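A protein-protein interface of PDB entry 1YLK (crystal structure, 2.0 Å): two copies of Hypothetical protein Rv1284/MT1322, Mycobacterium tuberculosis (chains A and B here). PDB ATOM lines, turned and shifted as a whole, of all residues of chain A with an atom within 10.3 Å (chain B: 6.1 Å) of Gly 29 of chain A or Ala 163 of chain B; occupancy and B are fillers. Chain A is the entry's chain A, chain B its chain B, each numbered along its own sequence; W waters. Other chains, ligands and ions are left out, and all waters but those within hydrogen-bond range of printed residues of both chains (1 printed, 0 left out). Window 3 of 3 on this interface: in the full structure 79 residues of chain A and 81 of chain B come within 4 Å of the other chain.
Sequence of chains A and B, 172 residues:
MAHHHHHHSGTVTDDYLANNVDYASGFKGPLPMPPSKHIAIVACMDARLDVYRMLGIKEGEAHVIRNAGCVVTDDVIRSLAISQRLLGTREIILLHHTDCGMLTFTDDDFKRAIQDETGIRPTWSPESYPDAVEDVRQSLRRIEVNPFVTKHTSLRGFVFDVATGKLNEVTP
The side-chain hydroxyl (OH) of Tyr 23 of chain A sits at hydrogen-bond distance from the side-chain carboxylate (OE2) of Glu 59 of chain A (2.5 Å).
The backbone carbonyl oxygen (O) of Phe 160 of chain B is in hydrogen-bond range of the backbone NH (N) of Thr 98 of chain B (2.9 Å).
The backbone NH (N) of Ala 163 of chain B is in hydrogen-bond range of the side-chain carboxylate (OD1) of Asp 161 of chain B (3.1 Å).
The side-chain hydroxyl of Thr 98 of chain B is in hydrogen-bond range of the backbone NH of Val 162 of chain B, at 3.2 Å.
No position is printed for both chains.
Of the 12 pairs that touch across the chains among the printed residues, none has its exchanged pair printed and touching as well.
The backbone carbonyl oxygen of Ala 163 of chain B lies close to the backbone carbonyl oxygen of Gly 29 of chain A.
Ala 163 of chain B touches just these residues of chain A: Phe 27, Gly 29 and Pro 30.
Of chain A, only Phe 27, Gly 29 and Pro 30 come within 4 Å of Val 162 of chain B.
Thr 164 of chain B touches just these residues of chain A: Ala 24 (3.6 Å) and Phe 27 (3.3 Å).
Of the printed residues of chain B, Tyr 23 of chain A touches Phe 160 and Gly 165.
Of the printed residues of chain B, Pro 30 of chain A touches Val 162 (3.3 Å) and Ala 163 (3.8 Å).
Printed residues of chain B within 4 Å of Phe 27 of chain A: Val 162, Ala 163, Thr 164 and Gly 165.
Thr 98 of chain B touches none of the printed residues of chain A.
Glu 59 of chain A touches none of the printed residues of chain B.
The nearest residue of chain B that does not touch Gly 29 of chain A is Thr 164 of chain B (5.5 Å).
Among the printed residues, merely in contact across the chains: Tyr 23 of chain A with Phe 160 of chain B, Tyr 23 of chain A with Gly 165 of chain B, Ala 24 of chain A with Thr 164 of chain B, Ala 24 of chain A with Gly 165 of chain B, Phe 27 of chain A with Val 162 of chain B, Phe 27 of chain A with Ala 163 of chain B, Phe 27 of chain A with Thr 164 of chain B, Phe 27 of chain A with Gly 165 of chain B, Gly 29 of chain A with Val 162 of chain B, Pro 30 of chain A with Val 162 of chain B and Pro 30 of chain A with Ala 163 of chain B.
Water W1 bridges O of Val 162 of chain B and N of Leu 31 of chain A.
Of the 7 printed residues of chain B, 5 touch a printed residue of chain A.
Hydrophobic or aromatic side chains of chain B within 4 Å of the printed part of chain A: Phe 160 and Ala 163.
Along chain B the printed residues that touch a printed residue of chain A span positions 160 to 165.
Of the 12 printed residues of chain A, 5 touch a printed residue of chain B.
Printed residues of chain A that touch a printed residue of chain B: Tyr 23, Ala 24, Phe 27, Gly 29 and Pro 30.
Among the printed residues, 12 pairs touch across the chains.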
ATOM      1  N   TYR A  23     -31.452  -7.574   7.102  1.00  0.00           N
ATOM      2  CA  TYR A  23     -30.023  -7.799   7.311  1.00  0.00           C
ATOM      3  C   TYR A  23     -29.185  -6.650   6.756  1.00  0.00           C
ATOM      4  O   TYR A  23     -28.264  -6.176   7.423  1.00  0.00           O
ATOM      5  CB  TYR A  23     -29.578  -9.134   6.692  1.00  0.00           C
ATOM      6  CG  TYR A  23     -28.083  -9.368   6.747  1.00  0.00           C
ATOM      7  CD1 TYR A  23     -27.467  -9.867   7.904  1.00  0.00           C
ATOM      8  CD2 TYR A  23     -27.280  -9.103   5.640  1.00  0.00           C
ATOM      9  CE1 TYR A  23     -26.083 -10.089   7.949  1.00  0.00           C
ATOM     10  CE2 TYR A  23     -25.915  -9.316   5.682  1.00  0.00           C
ATOM     11  CZ  TYR A  23     -25.324  -9.807   6.832  1.00  0.00           C
ATOM     12  OH  TYR A  23     -23.968 -10.005   6.846  1.00  0.00           O
ATOM     13  N   ALA A  24     -29.508  -6.216   5.537  1.00  0.00           N
ATOM     14  CA  ALA A  24     -28.776  -5.147   4.867  1.00  0.00           C
ATOM     15  C   ALA A  24     -28.888  -3.771   5.548  1.00  0.00           C
ATOM     16  O   ALA A  24     -27.954  -2.975   5.462  1.00  0.00           O
ATOM     17  CB  ALA A  24     -29.197  -5.058   3.397  1.00  0.00           C
ATOM     18  N   SER A  25     -30.012  -3.492   6.216  1.00  0.00           N
ATOM     19  CA  SER A  25     -30.186  -2.204   6.910  1.00  0.00           C
ATOM     20  C   SER A  25     -29.173  -2.008   8.043  1.00  0.00           C
ATOM     21  O   SER A  25     -28.774  -0.881   8.335  1.00  0.00           O
ATOM     22  CB  SER A  25     -31.621  -2.020   7.425  1.00  0.00           C
ATOM     23  OG  SER A  25     -31.963  -3.005   8.386  1.00  0.00           O
ATOM     24  N   GLY A  26     -28.751  -3.107   8.663  1.00  0.00           N
ATOM     25  CA  GLY A  26     -27.751  -3.053   9.730  1.00  0.00           C
ATOM     26  C   GLY A  26     -26.420  -3.675   9.346  1.00  0.00           C
ATOM     27  O   GLY A  26     -25.696  -4.185  10.211  1.00  0.00           O
ATOM     28  N   PHE A  27     -26.098  -3.637   8.052  1.00  0.00           N
ATOM     29  CA  PHE A  27     -24.852  -4.223   7.552  1.00  0.00           C
ATOM     30  C   PHE A  27     -23.692  -3.228   7.548  1.00  0.00           C
ATOM     31  O   PHE A  27     -23.834  -2.072   7.151  1.00  0.00           O
ATOM     32  CB  PHE A  27     -25.039  -4.811   6.149  1.00  0.00           C
ATOM     33  CG  PHE A  27     -23.794  -5.428   5.574  1.00  0.00           C
ATOM     34  CD1 PHE A  27     -23.439  -6.729   5.893  1.00  0.00           C
ATOM     35  CD2 PHE A  27     -22.968  -4.701   4.727  1.00  0.00           C
ATOM     36  CE1 PHE A  27     -22.299  -7.306   5.367  1.00  0.00           C
ATOM     37  CE2 PHE A  27     -21.815  -5.267   4.200  1.00  0.00           C
ATOM     38  CZ  PHE A  27     -21.483  -6.574   4.521  1.00  0.00           C
ATOM     39  N   LYS A  28     -22.538  -3.727   7.966  1.00  0.00           N
ATOM     40  CA  LYS A  28     -21.296  -2.972   8.002  1.00  0.00           C
ATOM     41  C   LYS A  28     -20.236  -3.714   7.176  1.00  0.00           C
ATOM     42  O   LYS A  28     -19.855  -4.851   7.475  1.00  0.00           O
ATOM     43  CB  LYS A  28     -20.862  -2.772   9.462  1.00  0.00           C
ATOM     44  CG  LYS A  28     -21.124  -4.007  10.339  1.00  0.00           C
ATOM     45  CD  LYS A  28     -21.938  -3.652  11.577  1.00  0.00           C
ATOM     46  CE  LYS A  28     -22.674  -4.889  12.101  1.00  0.00           C
ATOM     47  NZ  LYS A  28     -23.618  -4.562  13.221  1.00  0.00           N
ATOM     48  N   GLY A  29     -19.794  -3.068   6.105  1.00  0.00           N
ATOM     49  CA  GLY A  29     -18.816  -3.653   5.198  1.00  0.00           C
ATOM     50  C   GLY A  29     -18.397  -2.602   4.190  1.00  0.00           C
ATOM     51  O   GLY A  29     -18.933  -1.494   4.204  1.00  0.00           O
ATOM     52  N   PRO A  30     -17.468  -2.943   3.286  1.00  0.00           N
ATOM     53  CA  PRO A  30     -16.870  -4.262   3.114  1.00  0.00           C
ATOM     54  C   PRO A  30     -15.791  -4.607   4.145  1.00  0.00           C
ATOM     55  O   PRO A  30     -15.208  -3.719   4.783  1.00  0.00           O
ATOM     56  CB  PRO A  30     -16.259  -4.176   1.715  1.00  0.00           C
ATOM     57  CG  PRO A  30     -15.881  -2.750   1.574  1.00  0.00           C
ATOM     58  CD  PRO A  30     -16.951  -1.978   2.298  1.00  0.00           C
ATOM     59  N   LEU A  31     -15.557  -5.905   4.304  1.00  0.00           N
ATOM     60  CA  LEU A  31     -14.424  -6.422   5.059  1.00  0.00           C
ATOM     61  C   LEU A  31     -13.369  -6.864   4.050  1.00  0.00           C
ATOM     62  O   LEU A  31     -13.683  -6.993   2.866  1.00  0.00           O
ATOM     63  CB  LEU A  31     -14.866  -7.601   5.948  1.00  0.00           C
ATOM     64  CG  LEU A  31     -15.869  -7.243   7.050  1.00  0.00           C
ATOM     65  CD1 LEU A  31     -16.150  -8.438   7.931  1.00  0.00           C
ATOM     66  CD2 LEU A  31     -15.387  -6.054   7.880  1.00  0.00           C
ATOM     67  N   PRO A  32     -12.107  -7.059   4.497  1.00  0.00           N
ATOM     68  CA  PRO A  32     -11.089  -7.659   3.622  1.00  0.00           C
ATOM     69  C   PRO A  32     -11.438  -9.087   3.210  1.00  0.00           C
ATOM     70  O   PRO A  32     -12.161  -9.783   3.929  1.00  0.00           O
ATOM     71  CB  PRO A  32      -9.831  -7.674   4.500  1.00  0.00           C
ATOM     72  CG  PRO A  32     -10.085  -6.667   5.560  1.00  0.00           C
ATOM     73  CD  PRO A  32     -11.551  -6.698   5.815  1.00  0.00           C
ATOM     74  N   GLU A  59     -18.316 -12.378  11.262  1.00  0.00           N
ATOM     75  CA  GLU A  59     -18.101 -12.070   9.850  1.00  0.00           C
ATOM     76  C   GLU A  59     -16.651 -11.729   9.560  1.00  0.00           C
ATOM     77  O   GLU A  59     -16.025 -10.983  10.303  1.00  0.00           O
ATOM     78  CB  GLU A  59     -19.023 -10.931   9.387  1.00  0.00           C
ATOM     79  CG  GLU A  59     -20.473 -11.400   9.151  1.00  0.00           C
ATOM     80  CD  GLU A  59     -21.426 -10.267   8.776  1.00  0.00           C
ATOM     81  OE1 GLU A  59     -20.970  -9.207   8.309  1.00  0.00           O
ATOM     82  OE2 GLU A  59     -22.649 -10.449   8.945  1.00  0.00           O
ATOM     83  N   GLY A  60     -16.123 -12.309   8.488  1.00  0.00           N
ATOM     84  CA  GLY A  60     -14.801 -11.960   7.991  1.00  0.00           C
ATOM     85  C   GLY A  60     -13.670 -12.781   8.567  1.00  0.00           C
ATOM     86  O   GLY A  60     -12.523 -12.593   8.172  1.00  0.00           O
ATOM     87  N   THR B  98     -19.937 -10.192  -4.776  1.00  0.00           N
ATOM     88  CA  THR B  98     -18.968  -9.239  -5.313  1.00  0.00           C
ATOM     89  C   THR B  98     -17.657  -9.374  -4.537  1.00  0.00           C
ATOM     90  O   THR B  98     -17.657  -9.807  -3.380  1.00  0.00           O
ATOM     91  CB  THR B  98     -19.473  -7.795  -5.152  1.00  0.00           C
ATOM     92  OG1 THR B  98     -19.570  -7.494  -3.761  1.00  0.00           O
ATOM     93  CG2 THR B  98     -20.836  -7.613  -5.815  1.00  0.00           C
ATOM     94  N   PHE B 160     -24.442 -11.374  -3.821  1.00  0.00           N
ATOM     95  CA  PHE B 160     -24.360 -10.675  -2.550  1.00  0.00           C
ATOM     96  C   PHE B 160     -23.303  -9.550  -2.616  1.00  0.00           C
ATOM     97  O   PHE B 160     -22.146  -9.786  -2.958  1.00  0.00           O
ATOM     98  CB  PHE B 160     -24.009 -11.702  -1.445  1.00  0.00           C
ATOM     99  CG  PHE B 160     -23.810 -11.098  -0.076  1.00  0.00           C
ATOM    100  CD1 PHE B 160     -24.903 -10.694   0.690  1.00  0.00           C
ATOM    101  CD2 PHE B 160     -22.526 -10.966   0.459  1.00  0.00           C
ATOM    102  CE1 PHE B 160     -24.722 -10.159   1.972  1.00  0.00           C
ATOM    103  CE2 PHE B 160     -22.335 -10.416   1.733  1.00  0.00           C
ATOM    104  CZ  PHE B 160     -23.435 -10.004   2.483  1.00  0.00           C
ATOM    105  N   ASP B 161     -23.719  -8.325  -2.316  1.00  0.00           N
ATOM    106  CA  ASP B 161     -22.804  -7.195  -2.290  1.00  0.00           C
ATOM    107  C   ASP B 161     -22.125  -7.133  -0.909  1.00  0.00           C
ATOM    108  O   ASP B 161     -22.779  -6.855   0.101  1.00  0.00           O
ATOM    109  CB  ASP B 161     -23.559  -5.899  -2.651  1.00  0.00           C
ATOM    110  CG  ASP B 161     -22.632  -4.746  -2.992  1.00  0.00           C
ATOM    111  OD1 ASP B 161     -21.527  -4.669  -2.428  1.00  0.00           O
ATOM    112  OD2 ASP B 161     -23.009  -3.899  -3.832  1.00  0.00           O
ATOM    113  N   VAL B 162     -20.819  -7.415  -0.865  1.00  0.00           N
ATOM    114  CA  VAL B 162     -20.085  -7.479   0.412  1.00  0.00           C
ATOM    115  C   VAL B 162     -19.918  -6.109   1.070  1.00  0.00           C
ATOM    116  O   VAL B 162     -19.494  -6.034   2.223  1.00  0.00           O
ATOM    117  CB  VAL B 162     -18.683  -8.167   0.274  1.00  0.00           C
ATOM    118  CG1 VAL B 162     -18.830  -9.612  -0.185  1.00  0.00           C
ATOM    119  CG2 VAL B 162     -17.775  -7.380  -0.664  1.00  0.00           C
ATOM    120  N   ALA B 163     -20.241  -5.045   0.325  1.00  0.00           N
ATOM    121  CA  ALA B 163     -20.218  -3.664   0.822  1.00  0.00           C
ATOM    122  C   ALA B 163     -21.550  -3.193   1.418  1.00  0.00           C
ATOM    123  O   ALA B 163     -21.551  -2.370   2.335  1.00  0.00           O
ATOM    124  CB  ALA B 163     -19.786  -2.707  -0.279  1.00  0.00           C
ATOM    125  N   THR B 164     -22.670  -3.703   0.902  1.00  0.00           N
ATOM    126  CA  THR B 164     -24.003  -3.247   1.324  1.00  0.00           C
ATOM    127  C   THR B 164     -24.806  -4.329   2.047  1.00  0.00           C
ATOM    128  O   THR B 164     -25.755  -4.028   2.772  1.00  0.00           O
ATOM    129  CB  THR B 164     -24.862  -2.772   0.131  1.00  0.00           C
ATOM    130  OG1 THR B 164     -25.162  -3.890  -0.718  1.00  0.00           O
ATOM    131  CG2 THR B 164     -24.150  -1.684  -0.667  1.00  0.00           C
ATOM    132  N   GLY B 165     -24.433  -5.589   1.824  1.00  0.00           N
ATOM    133  CA  GLY B 165     -25.131  -6.723   2.413  1.00  0.00           C
ATOM    134  C   GLY B 165     -26.410  -7.090   1.681  1.00  0.00           C
ATOM    135  O   GLY B 165     -27.200  -7.881   2.181  1.00  0.00           O
HETATM  136  O   HOH W   1     -17.954  -7.371   3.783  1.00  0.00           O
